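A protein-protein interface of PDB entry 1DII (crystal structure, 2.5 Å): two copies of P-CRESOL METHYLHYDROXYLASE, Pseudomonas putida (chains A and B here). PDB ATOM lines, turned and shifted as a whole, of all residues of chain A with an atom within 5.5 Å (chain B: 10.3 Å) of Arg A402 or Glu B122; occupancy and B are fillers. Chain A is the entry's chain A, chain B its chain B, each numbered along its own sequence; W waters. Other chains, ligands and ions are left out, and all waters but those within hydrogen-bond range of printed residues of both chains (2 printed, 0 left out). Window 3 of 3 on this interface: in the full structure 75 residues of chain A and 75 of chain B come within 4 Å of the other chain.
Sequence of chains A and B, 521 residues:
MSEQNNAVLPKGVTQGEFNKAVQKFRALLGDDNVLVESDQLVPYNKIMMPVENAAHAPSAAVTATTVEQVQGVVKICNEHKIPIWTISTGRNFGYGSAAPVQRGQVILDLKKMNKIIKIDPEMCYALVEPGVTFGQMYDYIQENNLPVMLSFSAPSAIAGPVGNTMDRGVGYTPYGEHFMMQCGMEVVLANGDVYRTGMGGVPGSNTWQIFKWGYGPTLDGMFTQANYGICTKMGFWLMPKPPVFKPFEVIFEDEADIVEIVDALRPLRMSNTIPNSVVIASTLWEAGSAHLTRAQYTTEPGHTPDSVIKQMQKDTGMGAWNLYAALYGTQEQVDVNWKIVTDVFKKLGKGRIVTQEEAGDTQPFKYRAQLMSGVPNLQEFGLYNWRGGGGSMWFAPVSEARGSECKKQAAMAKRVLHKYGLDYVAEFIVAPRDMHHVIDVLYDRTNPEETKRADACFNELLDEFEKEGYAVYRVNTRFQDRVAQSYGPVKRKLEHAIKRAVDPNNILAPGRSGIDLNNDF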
ATOM      1  N   VAL A 262      -4.796 -21.893 -22.756  1.00  0.00           N
ATOM      2  CA  VAL A 262      -3.738 -21.429 -21.867  1.00  0.00           C
ATOM      3  C   VAL A 262      -4.215 -21.232 -20.432  1.00  0.00           C
ATOM      4  O   VAL A 262      -3.600 -21.776 -19.520  1.00  0.00           O
ATOM      5  CB  VAL A 262      -3.051 -20.164 -22.446  1.00  0.00           C
ATOM      6  CG1 VAL A 262      -2.028 -19.597 -21.486  1.00  0.00           C
ATOM      7  CG2 VAL A 262      -2.383 -20.506 -23.766  1.00  0.00           C
ATOM      8  N   ASP A 263      -5.356 -20.557 -20.254  1.00  0.00           N
ATOM      9  CA  ASP A 263      -5.940 -20.312 -18.927  1.00  0.00           C
ATOM     10  C   ASP A 263      -6.404 -21.589 -18.215  1.00  0.00           C
ATOM     11  O   ASP A 263      -6.375 -21.667 -16.988  1.00  0.00           O
ATOM     12  CB  ASP A 263      -7.074 -19.290 -19.014  1.00  0.00           C
ATOM     13  CG  ASP A 263      -6.573 -17.877 -19.332  1.00  0.00           C
ATOM     14  OD1 ASP A 263      -5.472 -17.501 -18.881  1.00  0.00           O
ATOM     15  OD2 ASP A 263      -7.275 -17.122 -20.032  1.00  0.00           O
ATOM     16  N   ARG A 266      -2.726 -23.634 -17.342  1.00  0.00           N
ATOM     17  CA  ARG A 266      -1.860 -23.017 -16.339  1.00  0.00           C
ATOM     18  C   ARG A 266      -1.900 -23.688 -14.950  1.00  0.00           C
ATOM     19  O   ARG A 266      -0.833 -24.057 -14.462  1.00  0.00           O
ATOM     20  CB  ARG A 266      -2.064 -21.487 -16.301  1.00  0.00           C
ATOM     21  CG  ARG A 266      -1.223 -20.746 -15.278  1.00  0.00           C
ATOM     22  CD  ARG A 266      -1.652 -19.303 -15.133  1.00  0.00           C
ATOM     23  NE  ARG A 266      -3.064 -19.184 -14.780  1.00  0.00           N
ATOM     24  CZ  ARG A 266      -3.951 -18.480 -15.477  1.00  0.00           C
ATOM     25  NH1 ARG A 266      -3.574 -17.824 -16.570  1.00  0.00           N
ATOM     26  NH2 ARG A 266      -5.222 -18.459 -15.101  1.00  0.00           N
ATOM     27  N   MET A 270       1.224 -25.498 -13.226  1.00  0.00           N
ATOM     28  CA  MET A 270       1.757 -24.903 -12.003  1.00  0.00           C
ATOM     29  C   MET A 270       1.771 -25.868 -10.818  1.00  0.00           C
ATOM     30  O   MET A 270       2.586 -25.721  -9.901  1.00  0.00           O
ATOM     31  CB  MET A 270       0.952 -23.664 -11.634  1.00  0.00           C
ATOM     32  CG  MET A 270       1.809 -22.531 -11.180  1.00  0.00           C
ATOM     33  SD  MET A 270       0.835 -21.232 -10.538  1.00  0.00           S
ATOM     34  CE  MET A 270       0.783 -20.140 -11.854  1.00  0.00           C
ATOM     35  N   SER A 399       5.976 -13.675 -21.985  1.00  0.00           N
ATOM     36  CA  SER A 399       4.799 -13.086 -21.351  1.00  0.00           C
ATOM     37  C   SER A 399       4.306 -13.995 -20.239  1.00  0.00           C
ATOM     38  O   SER A 399       4.797 -15.114 -20.080  1.00  0.00           O
ATOM     39  CB  SER A 399       3.650 -12.890 -22.381  1.00  0.00           C
ATOM     40  OG  SER A 399       2.975 -14.114 -22.698  1.00  0.00           O
ATOM     41  N   GLU A 400       3.299 -13.517 -19.504  1.00  0.00           N
ATOM     42  CA  GLU A 400       2.639 -14.298 -18.468  1.00  0.00           C
ATOM     43  C   GLU A 400       1.888 -15.421 -19.187  1.00  0.00           C
ATOM     44  O   GLU A 400       1.392 -15.215 -20.312  1.00  0.00           O
ATOM     45  CB  GLU A 400       1.541 -13.489 -17.785  1.00  0.00           C
ATOM     46  CG  GLU A 400       1.902 -12.169 -17.151  1.00  0.00           C
ATOM     47  CD  GLU A 400       0.772 -11.670 -16.248  1.00  0.00           C
ATOM     48  OE1 GLU A 400       1.005 -11.545 -15.028  1.00  0.00           O
ATOM     49  OE2 GLU A 400      -0.360 -11.437 -16.750  1.00  0.00           O
ATOM     50  N   ALA A 401       1.735 -16.572 -18.527  1.00  0.00           N
ATOM     51  CA  ALA A 401       1.001 -17.702 -19.117  1.00  0.00           C
ATOM     52  C   ALA A 401      -0.496 -17.460 -18.956  1.00  0.00           C
ATOM     53  O   ALA A 401      -1.229 -18.224 -18.315  1.00  0.00           O
ATOM     54  CB  ALA A 401       1.431 -19.013 -18.502  1.00  0.00           C
ATOM     55  N   ARG A 402      -0.912 -16.353 -19.571  1.00  0.00           N
ATOM     56  CA  ARG A 402      -2.284 -15.858 -19.580  1.00  0.00           C
ATOM     57  C   ARG A 402      -2.814 -15.926 -21.019  1.00  0.00           C
ATOM     58  O   ARG A 402      -2.134 -15.477 -21.949  1.00  0.00           O
ATOM     59  CB  ARG A 402      -2.279 -14.403 -19.089  1.00  0.00           C
ATOM     60  CG  ARG A 402      -3.645 -13.797 -18.837  1.00  0.00           C
ATOM     61  CD  ARG A 402      -3.991 -13.760 -17.350  1.00  0.00           C
ATOM     62  NE  ARG A 402      -3.115 -12.858 -16.602  1.00  0.00           N
ATOM     63  CZ  ARG A 402      -3.245 -12.591 -15.303  1.00  0.00           C
ATOM     64  NH1 ARG A 402      -4.218 -13.156 -14.593  1.00  0.00           N
ATOM     65  NH2 ARG A 402      -2.387 -11.763 -14.708  1.00  0.00           N
ATOM     66  N   GLY A 403      -4.016 -16.490 -21.193  1.00  0.00           N
ATOM     67  CA  GLY A 403      -4.647 -16.605 -22.508  1.00  0.00           C
ATOM     68  C   GLY A 403      -4.877 -15.319 -23.308  1.00  0.00           C
ATOM     69  O   GLY A 403      -4.840 -15.335 -24.539  1.00  0.00           O
ATOM     70  N   SER A 404      -5.115 -14.206 -22.610  1.00  0.00           N
ATOM     71  CA  SER A 404      -5.339 -12.906 -23.244  1.00  0.00           C
ATOM     72  C   SER A 404      -4.064 -12.396 -23.912  1.00  0.00           C
ATOM     73  O   SER A 404      -4.119 -11.589 -24.836  1.00  0.00           O
ATOM     74  CB  SER A 404      -5.851 -11.876 -22.214  1.00  0.00           C
ATOM     75  OG  SER A 404      -4.857 -11.490 -21.268  1.00  0.00           O
ATOM     76  N   GLU A 405      -2.924 -12.906 -23.450  1.00  0.00           N
ATOM     77  CA  GLU A 405      -1.614 -12.522 -23.964  1.00  0.00           C
ATOM     78  C   GLU A 405      -1.302 -13.183 -25.294  1.00  0.00           C
ATOM     79  O   GLU A 405      -0.521 -12.656 -26.086  1.00  0.00           O
ATOM     80  CB  GLU A 405      -0.529 -12.839 -22.943  1.00  0.00           C
ATOM     81  CG  GLU A 405      -0.523 -11.936 -21.735  1.00  0.00           C
ATOM     82  CD  GLU A 405       0.159 -10.604 -21.993  1.00  0.00           C
ATOM     83  OE1 GLU A 405       0.023  -9.696 -21.142  1.00  0.00           O
ATOM     84  OE2 GLU A 405       0.838 -10.470 -23.036  1.00  0.00           O
ATOM     85  N   CYS A 406      -1.932 -14.330 -25.537  1.00  0.00           N
ATOM     86  CA  CYS A 406      -1.778 -15.065 -26.787  1.00  0.00           C
ATOM     87  C   CYS A 406      -2.397 -14.302 -27.954  1.00  0.00           C
ATOM     88  O   CYS A 406      -1.749 -14.090 -28.980  1.00  0.00           O
ATOM     89  CB  CYS A 406      -2.463 -16.410 -26.698  1.00  0.00           C
ATOM     90  SG  CYS A 406      -1.604 -17.614 -25.749  1.00  0.00           S
ATOM     91  N   MET A 435       5.246 -17.865 -20.514  1.00  0.00           N
ATOM     92  CA  MET A 435       4.822 -18.377 -21.812  1.00  0.00           C
ATOM     93  C   MET A 435       5.732 -17.710 -22.818  1.00  0.00           C
ATOM     94  O   MET A 435       5.996 -16.488 -22.752  1.00  0.00           O
ATOM     95  CB  MET A 435       3.373 -18.005 -22.104  1.00  0.00           C
ATOM     96  CG  MET A 435       2.766 -18.677 -23.302  1.00  0.00           C
ATOM     97  SD  MET A 435       1.005 -18.277 -23.495  1.00  0.00           S
ATOM     98  CE  MET A 435       0.969 -16.494 -23.703  1.00  0.00           C
ATOM     99  N   LYS B 118       2.875  -6.423  -3.941  1.00  0.00           N
ATOM    100  CA  LYS B 118       1.906  -7.172  -4.751  1.00  0.00           C
ATOM    101  C   LYS B 118       1.993  -8.670  -4.467  1.00  0.00           C
ATOM    102  O   LYS B 118       3.075  -9.197  -4.215  1.00  0.00           O
ATOM    103  CB  LYS B 118       2.189  -6.912  -6.253  1.00  0.00           C
ATOM    104  CG  LYS B 118       1.230  -7.514  -7.269  1.00  0.00           C
ATOM    105  CD  LYS B 118       1.352  -6.758  -8.619  1.00  0.00           C
ATOM    106  CE  LYS B 118       0.825  -7.564  -9.843  1.00  0.00           C
ATOM    107  NZ  LYS B 118      -0.531  -8.215  -9.718  1.00  0.00           N
ATOM    108  N   ILE B 119       0.833  -9.309  -4.357  1.00  0.00           N
ATOM    109  CA  ILE B 119       0.739 -10.760  -4.191  1.00  0.00           C
ATOM    110  C   ILE B 119      -0.313 -11.136  -5.220  1.00  0.00           C
ATOM    111  O   ILE B 119      -1.498 -10.843  -5.047  1.00  0.00           O
ATOM    112  CB  ILE B 119       0.299 -11.252  -2.768  1.00  0.00           C
ATOM    113  CG1 ILE B 119       1.366 -10.896  -1.722  1.00  0.00           C
ATOM    114  CG2 ILE B 119       0.083 -12.788  -2.782  1.00  0.00           C
ATOM    115  CD1 ILE B 119       1.061 -11.322  -0.332  1.00  0.00           C
ATOM    116  N   ASP B 120       0.145 -11.711  -6.328  1.00  0.00           N
ATOM    117  CA  ASP B 120      -0.726 -12.139  -7.423  1.00  0.00           C
ATOM    118  C   ASP B 120      -1.243 -13.549  -7.087  1.00  0.00           C
ATOM    119  O   ASP B 120      -0.454 -14.476  -6.937  1.00  0.00           O
ATOM    120  CB  ASP B 120       0.090 -12.140  -8.715  1.00  0.00           C
ATOM    121  CG  ASP B 120      -0.764 -12.109  -9.962  1.00  0.00           C
ATOM    122  OD1 ASP B 120      -1.589 -13.042 -10.128  1.00  0.00           O
ATOM    123  OD2 ASP B 120      -0.568 -11.170 -10.782  1.00  0.00           O
ATOM    124  N   PRO B 121      -2.567 -13.705  -6.883  1.00  0.00           N
ATOM    125  CA  PRO B 121      -3.102 -15.036  -6.553  1.00  0.00           C
ATOM    126  C   PRO B 121      -3.308 -15.974  -7.745  1.00  0.00           C
ATOM    127  O   PRO B 121      -3.541 -17.173  -7.563  1.00  0.00           O
ATOM    128  CB  PRO B 121      -4.410 -14.711  -5.833  1.00  0.00           C
ATOM    129  CG  PRO B 121      -4.866 -13.469  -6.536  1.00  0.00           C
ATOM    130  CD  PRO B 121      -3.601 -12.663  -6.715  1.00  0.00           C
ATOM    131  N   GLU B 122      -3.203 -15.418  -8.950  1.00  0.00           N
ATOM    132  CA  GLU B 122      -3.366 -16.184 -10.190  1.00  0.00           C
ATOM    133  C   GLU B 122      -2.021 -16.631 -10.756  1.00  0.00           C
ATOM    134  O   GLU B 122      -1.841 -17.815 -11.078  1.00  0.00           O
ATOM    135  CB  GLU B 122      -4.132 -15.371 -11.236  1.00  0.00           C
ATOM    136  CG  GLU B 122      -5.634 -15.268 -10.975  1.00  0.00           C
ATOM    137  CD  GLU B 122      -6.333 -14.463 -12.042  1.00  0.00           C
ATOM    138  OE1 GLU B 122      -6.682 -15.058 -13.084  1.00  0.00           O
ATOM    139  OE2 GLU B 122      -6.513 -13.236 -11.847  1.00  0.00           O
ATOM    140  N   MET B 123      -1.084 -15.689 -10.879  1.00  0.00           N
ATOM    141  CA  MET B 123       0.252 -16.020 -11.366  1.00  0.00           C
ATOM    142  C   MET B 123       1.127 -16.598 -10.261  1.00  0.00           C
ATOM    143  O   MET B 123       2.169 -17.182 -10.538  1.00  0.00           O
ATOM    144  CB  MET B 123       0.943 -14.827 -12.013  1.00  0.00           C
ATOM    145  CG  MET B 123       0.303 -14.320 -13.303  1.00  0.00           C
ATOM    146  SD  MET B 123      -0.236 -15.602 -14.461  1.00  0.00           S
ATOM    147  CE  MET B 123       1.224 -16.252 -14.995  1.00  0.00           C
ATOM    148  N   CYS B 124       0.655 -16.468  -9.017  1.00  0.00           N
ATOM    149  CA  CYS B 124       1.313 -16.964  -7.814  1.00  0.00           C
ATOM    150  C   CYS B 124       2.732 -16.467  -7.553  1.00  0.00           C
ATOM    151  O   CYS B 124       3.700 -17.210  -7.687  1.00  0.00           O
ATOM    152  CB  CYS B 124       1.203 -18.491  -7.725  1.00  0.00           C
ATOM    153  SG  CYS B 124      -0.503 -19.086  -7.604  1.00  0.00           S
ATOM    154  N   TYR B 125       2.829 -15.171  -7.270  1.00  0.00           N
ATOM    155  CA  TYR B 125       4.082 -14.530  -6.925  1.00  0.00           C
ATOM    156  C   TYR B 125       3.882 -13.427  -5.887  1.00  0.00           C
ATOM    157  O   TYR B 125       2.760 -12.974  -5.663  1.00  0.00           O
ATOM    158  CB  TYR B 125       4.825 -13.995  -8.166  1.00  0.00           C
ATOM    159  CG  TYR B 125       4.203 -12.848  -8.934  1.00  0.00           C
ATOM    160  CD1 TYR B 125       4.231 -11.513  -8.450  1.00  0.00           C
ATOM    161  CD2 TYR B 125       3.677 -13.065 -10.208  1.00  0.00           C
ATOM    162  CE1 TYR B 125       3.748 -10.434  -9.241  1.00  0.00           C
ATOM    163  CE2 TYR B 125       3.201 -11.994 -11.002  1.00  0.00           C
ATOM    164  CZ  TYR B 125       3.244 -10.697 -10.509  1.00  0.00           C
ATOM    165  OH  TYR B 125       2.812  -9.686 -11.313  1.00  0.00           O
ATOM    166  N   ALA B 126       4.992 -12.932  -5.346  1.00  0.00           N
ATOM    167  CA  ALA B 126       4.961 -11.860  -4.369  1.00  0.00           C
ATOM    168  C   ALA B 126       6.128 -10.939  -4.625  1.00  0.00           C
ATOM    169  O   ALA B 126       7.171 -11.409  -5.048  1.00  0.00           O
ATOM    170  CB  ALA B 126       5.035 -12.419  -2.980  1.00  0.00           C
ATOM    171  N   ASN B 145      -8.013 -14.036   1.979  1.00  0.00           N
ATOM    172  CA  ASN B 145      -8.368 -15.379   1.477  1.00  0.00           C
ATOM    173  C   ASN B 145      -7.706 -15.854   0.161  1.00  0.00           C
ATOM    174  O   ASN B 145      -8.345 -16.511  -0.676  1.00  0.00           O
ATOM    175  CB  ASN B 145      -9.901 -15.543   1.441  1.00  0.00           C
ATOM    176  CG  ASN B 145     -10.345 -17.000   1.595  1.00  0.00           C
ATOM    177  OD1 ASN B 145      -9.868 -17.720   2.473  1.00  0.00           O
ATOM    178  ND2 ASN B 145     -11.257 -17.435   0.728  1.00  0.00           N
ATOM    179  N   LEU B 146      -6.407 -15.563   0.023  1.00  0.00           N
ATOM    180  CA  LEU B 146      -5.619 -15.937  -1.156  1.00  0.00           C
ATOM    181  C   LEU B 146      -5.219 -17.416  -1.146  1.00  0.00           C
ATOM    182  O   LEU B 146      -4.751 -17.914  -0.125  1.00  0.00           O
ATOM    183  CB  LEU B 146      -4.369 -15.072  -1.249  1.00  0.00           C
ATOM    184  CG  LEU B 146      -4.566 -13.565  -1.188  1.00  0.00           C
ATOM    185  CD1 LEU B 146      -3.210 -12.929  -1.314  1.00  0.00           C
ATOM    186  CD2 LEU B 146      -5.504 -13.033  -2.269  1.00  0.00           C
ATOM    187  N   PRO B 147      -5.414 -18.144  -2.280  1.00  0.00           N
ATOM    188  CA  PRO B 147      -5.055 -19.575  -2.342  1.00  0.00           C
ATOM    189  C   PRO B 147      -3.552 -19.863  -2.565  1.00  0.00           C
ATOM    190  O   PRO B 147      -3.169 -20.685  -3.411  1.00  0.00           O
ATOM    191  CB  PRO B 147      -5.945 -20.099  -3.480  1.00  0.00           C
ATOM    192  CG  PRO B 147      -5.946 -18.939  -4.435  1.00  0.00           C
ATOM    193  CD  PRO B 147      -6.121 -17.735  -3.518  1.00  0.00           C
ATOM    194  N   VAL B 148      -2.710 -19.161  -1.811  1.00  0.00           N
ATOM    195  CA  VAL B 148      -1.269 -19.355  -1.881  1.00  0.00           C
ATOM    196  C   VAL B 148      -0.732 -19.910  -0.567  1.00  0.00           C
ATOM    197  O   VAL B 148      -1.346 -19.769   0.481  1.00  0.00           O
ATOM    198  CB  VAL B 148      -0.484 -18.060  -2.258  1.00  0.00           C
ATOM    199  CG1 VAL B 148      -0.709 -17.690  -3.688  1.00  0.00           C
ATOM    200  CG2 VAL B 148      -0.850 -16.915  -1.369  1.00  0.00           C
ATOM    201  N   TYR B 175       8.566 -25.644  -2.334  1.00  0.00           N
ATOM    202  CA  TYR B 175       9.218 -24.405  -2.752  1.00  0.00           C
ATOM    203  C   TYR B 175      10.304 -24.041  -1.733  1.00  0.00           C
ATOM    204  O   TYR B 175      10.751 -22.885  -1.659  1.00  0.00           O
ATOM    205  CB  TYR B 175       8.186 -23.282  -2.860  1.00  0.00           C
ATOM    206  CG  TYR B 175       7.390 -23.262  -4.163  1.00  0.00           C
ATOM    207  CD1 TYR B 175       7.170 -22.051  -4.856  1.00  0.00           C
ATOM    208  CD2 TYR B 175       6.870 -24.453  -4.735  1.00  0.00           C
ATOM    209  CE1 TYR B 175       6.453 -22.033  -6.097  1.00  0.00           C
ATOM    210  CE2 TYR B 175       6.160 -24.434  -5.962  1.00  0.00           C
ATOM    211  CZ  TYR B 175       5.956 -23.227  -6.630  1.00  0.00           C
ATOM    212  OH  TYR B 175       5.237 -23.211  -7.810  1.00  0.00           O
ATOM    213  N   ASN B 206       5.477  -6.508 -17.308  1.00  0.00           N
ATOM    214  CA  ASN B 206       4.737  -7.112 -16.219  1.00  0.00           C
ATOM    215  C   ASN B 206       5.316  -8.515 -15.997  1.00  0.00           C
ATOM    216  O   ASN B 206       4.674  -9.384 -15.396  1.00  0.00           O
ATOM    217  CB  ASN B 206       3.237  -7.126 -16.542  1.00  0.00           C
ATOM    218  CG  ASN B 206       2.874  -8.021 -17.730  1.00  0.00           C
ATOM    219  OD1 ASN B 206       3.687  -8.258 -18.632  1.00  0.00           O
ATOM    220  ND2 ASN B 206       1.636  -8.527 -17.726  1.00  0.00           N
ATOM    221  N   THR B 207       6.553  -8.711 -16.459  1.00  0.00           N
ATOM    222  CA  THR B 207       7.231 -10.010 -16.359  1.00  0.00           C
ATOM    223  C   THR B 207       8.381 -10.231 -15.352  1.00  0.00           C
ATOM    224  O   THR B 207       8.949 -11.330 -15.305  1.00  0.00           O
ATOM    225  CB  THR B 207       7.691 -10.538 -17.762  1.00  0.00           C
ATOM    226  OG1 THR B 207       8.324  -9.487 -18.498  1.00  0.00           O
ATOM    227  CG2 THR B 207       6.534 -11.094 -18.548  1.00  0.00           C
ATOM    228  N   GLN B 209       8.511 -10.849 -12.158  1.00  0.00           N
ATOM    229  CA  GLN B 209       8.326 -11.974 -11.261  1.00  0.00           C
ATOM    230  C   GLN B 209       7.791 -13.171 -12.031  1.00  0.00           C
ATOM    231  O   GLN B 209       7.255 -14.113 -11.435  1.00  0.00           O
ATOM    232  CB  GLN B 209       7.376 -11.588 -10.133  1.00  0.00           C
ATOM    233  CG  GLN B 209       7.972 -10.859  -8.929  1.00  0.00           C
ATOM    234  CD  GLN B 209       8.552  -9.481  -9.237  1.00  0.00           C
ATOM    235  OE1 GLN B 209       7.822  -8.515  -9.457  1.00  0.00           O
ATOM    236  NE2 GLN B 209       9.866  -9.393  -9.254  1.00  0.00           N
ATOM    237  N   ILE B 210       7.976 -13.153 -13.356  1.00  0.00           N
ATOM    238  CA  ILE B 210       7.483 -14.224 -14.231  1.00  0.00           C
ATOM    239  C   ILE B 210       8.623 -15.013 -14.894  1.00  0.00           C
ATOM    240  O   ILE B 210       8.605 -16.251 -14.886  1.00  0.00           O
ATOM    241  CB  ILE B 210       6.470 -13.646 -15.308  1.00  0.00           C
ATOM    242  CG1 ILE B 210       5.210 -13.030 -14.658  1.00  0.00           C
ATOM    243  CG2 ILE B 210       6.078 -14.676 -16.334  1.00  0.00           C
ATOM    244  CD1 ILE B 210       4.276 -14.027 -13.940  1.00  0.00           C
ATOM    245  N   TRP B 237       8.338 -16.743  -6.140  1.00  0.00           N
ATOM    246  CA  TRP B 237       7.182 -17.555  -6.464  1.00  0.00           C
ATOM    247  C   TRP B 237       6.562 -18.191  -5.223  1.00  0.00           C
ATOM    248  O   TRP B 237       7.264 -18.506  -4.265  1.00  0.00           O
ATOM    249  CB  TRP B 237       7.569 -18.624  -7.475  1.00  0.00           C
ATOM    250  CG  TRP B 237       8.043 -18.079  -8.806  1.00  0.00           C
ATOM    251  CD1 TRP B 237       7.691 -16.882  -9.403  1.00  0.00           C
ATOM    252  CD2 TRP B 237       9.013 -18.683  -9.672  1.00  0.00           C
ATOM    253  NE1 TRP B 237       8.393 -16.706 -10.574  1.00  0.00           N
ATOM    254  CE2 TRP B 237       9.216 -17.784 -10.768  1.00  0.00           C
ATOM    255  CE3 TRP B 237       9.752 -19.896  -9.627  1.00  0.00           C
ATOM    256  CZ2 TRP B 237      10.136 -18.056 -11.811  1.00  0.00           C
ATOM    257  CZ3 TRP B 237      10.675 -20.174 -10.667  1.00  0.00           C
ATOM    258  CH2 TRP B 237      10.854 -19.250 -11.744  1.00  0.00           C
ATOM    259  N   LEU B 238       5.233 -18.312  -5.235  1.00  0.00           N
ATOM    260  CA  LEU B 238       4.459 -18.897  -4.136  1.00  0.00           C
ATOM    261  C   LEU B 238       3.770 -20.144  -4.638  1.00  0.00           C
ATOM    262  O   LEU B 238       3.282 -20.179  -5.769  1.00  0.00           O
ATOM    263  CB  LEU B 238       3.390 -17.920  -3.634  1.00  0.00           C
ATOM    264  CG  LEU B 238       3.870 -16.611  -3.044  1.00  0.00           C
ATOM    265  CD1 LEU B 238       2.728 -15.642  -2.920  1.00  0.00           C
ATOM    266  CD2 LEU B 238       4.515 -16.889  -1.713  1.00  0.00           C
ATOM    267  N   MET B 239       3.744 -21.177  -3.810  1.00  0.00           N
ATOM    268  CA  MET B 239       3.103 -22.434  -4.179  1.00  0.00           C
ATOM    269  C   MET B 239       1.589 -22.316  -4.089  1.00  0.00           C
ATOM    270  O   MET B 239       1.078 -21.722  -3.129  1.00  0.00           O
ATOM    271  CB  MET B 239       3.559 -23.568  -3.250  1.00  0.00           C
ATOM    272  CG  MET B 239       3.119 -24.953  -3.712  1.00  0.00           C
ATOM    273  SD  MET B 239       3.681 -26.325  -2.695  1.00  0.00           S
ATOM    274  CE  MET B 239       2.246 -27.197  -2.469  1.00  0.00           C
ATOM    275  N   PRO B 240       0.852 -22.774  -5.133  1.00  0.00           N
ATOM    276  CA  PRO B 240      -0.608 -22.678  -5.022  1.00  0.00           C
ATOM    277  C   PRO B 240      -1.040 -23.665  -3.921  1.00  0.00           C
ATOM    278  O   PRO B 240      -0.417 -24.726  -3.765  1.00  0.00           O
ATOM    279  CB  PRO B 240      -1.088 -23.112  -6.416  1.00  0.00           C
ATOM    280  CG  PRO B 240       0.039 -23.916  -6.961  1.00  0.00           C
ATOM    281  CD  PRO B 240       1.228 -23.128  -6.514  1.00  0.00           C
ATOM    282  N   LYS B 241      -2.000 -23.257  -3.093  1.00  0.00           N
ATOM    283  CA  LYS B 241      -2.491 -24.093  -2.003  1.00  0.00           C
ATOM    284  C   LYS B 241      -3.126 -25.355  -2.579  1.00  0.00           C
ATOM    285  O   LYS B 241      -3.992 -25.267  -3.450  1.00  0.00           O
ATOM    286  CB  LYS B 241      -3.507 -23.313  -1.164  1.00  0.00           C
ATOM    287  CG  LYS B 241      -3.725 -23.802   0.269  1.00  0.00           C
ATOM    288  CD  LYS B 241      -4.540 -22.759   1.034  1.00  0.00           C
ATOM    289  CE  LYS B 241      -4.676 -23.078   2.513  1.00  0.00           C
ATOM    290  NZ  LYS B 241      -5.198 -21.886   3.247  1.00  0.00           N
HETATM  291  O   HOH W   1       2.612  -9.544 -14.144  1.00  0.00           O
HETATM  292  O   HOH W   2       3.162 -10.335 -19.845  1.00  0.00           O
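NH1 of Arg A402 lies within salt-bridge range of OE1 of Glu B122 (3.5 Å).
The side-chain carboxylate (OD1) of Asp B120 lies within hydrogen-bond range of the backbone NH (N) of Glu B122 (3.1 Å).
O of Ser A399 sits at hydrogen-bond distance from N of Met A435 (2.8 Å).
NH1 of Arg A266 lies within hydrogen-bond range of O of Ala A401 (3.0 Å).
The side-chain carboxylate (OD1) of Asp B120 lies within hydrogen-bond range of the backbone NH (N) of Met B123 (2.8 Å).
O of Cys B124 lies within hydrogen-bond range of N of Leu B238, 3.1 Å away.
OE2 of Glu A400 lies within salt-bridge range of NH2 of Arg A402 (2.9 Å).
Glu B122 touches Met A270 (O to CE, 3.6 Å).
Met B123 touches Met A270.
SD of Met A270 touches SG of Cys B124 (3.9 Å).
Thr B207 touches Ser A399.
O of Ser A399 touches CG2 of Ile B210 (3.98 Å).
CG of Met B123 touches OE1 of Glu A400, 3.3 Å away.
Glu A400 touches Asn B206.
Ala A401 touches Met B123 (N to CE, 3.6 Å).
Met B123 touches Arg A402 (CG to NH2, 3.97 Å).
ND2 of Asn B206 touches OE1 of Glu A405, 3.95 Å away.
Of chain B, only Glu B122 (3.5 Å) and Met B123 (3.97 Å) come within 4 Å of Arg A402.
Ala A401 touches one residue of chain B.
No residue of chain B comes within 4 Å of Gly A403.
No residue of chain B comes within 4 Å of Ser A404.
Printed residues of chain B within 4 Å of Ser A399: Thr B207 (3.9 Å) and Ile B210 (3.98 Å).
Of the printed residues of chain A, Cys B124 touches Met A270.
Of the printed residues of chain A, Met B123 touches Met A270, Glu A400, Ala A401 and Arg A402.
Of the printed residues of chain A, Ile B210 touches Ser A399 (3.98 Å).
Printed residues of chain B within 4 Å of Met A270: Glu B122, Met B123 and Cys B124.
The nearest residue of chain B that does not touch Arg A402 is Asp B120 (4.4 Å).
The nearest residue of chain A that does not touch Glu B122 is Arg A266 (4.1 Å).
Of the 13 printed residues of chain A, 6 touch a printed residue of chain B.
Printed residues of chain A that touch a printed residue of chain B: Met A270, Ser A399, Glu A400, Ala A401, Arg A402 and Glu A405.
Along chain A the printed residues that touch a printed residue of chain B span positions 270 to 405.
Hydrophobic or aromatic side chains of chain B that line the printed part of chain A: Met B123 and Ile B210.
Along chain B the printed residues that touch a printed residue of chain A span positions 122 to 210.
Among the printed residues, 11 pairs touch across the chains.
No position is printed for both chains.
Of the 11 pairs that touch across the chains among the printed residues, none has its exchanged pair printed and touching as well.
Water W1 lies within hydrogen-bond range of O of Asn B206, OE1 of Glu A400 and OH of Tyr B125.
Water W2 lies within hydrogen-bond range of the side-chain amide oxygen of Asn B206 (2.5 Å), the backbone NH of Glu A400 (3.2 Å) and the side-chain carboxylate of Glu A405 (3.5 Å).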
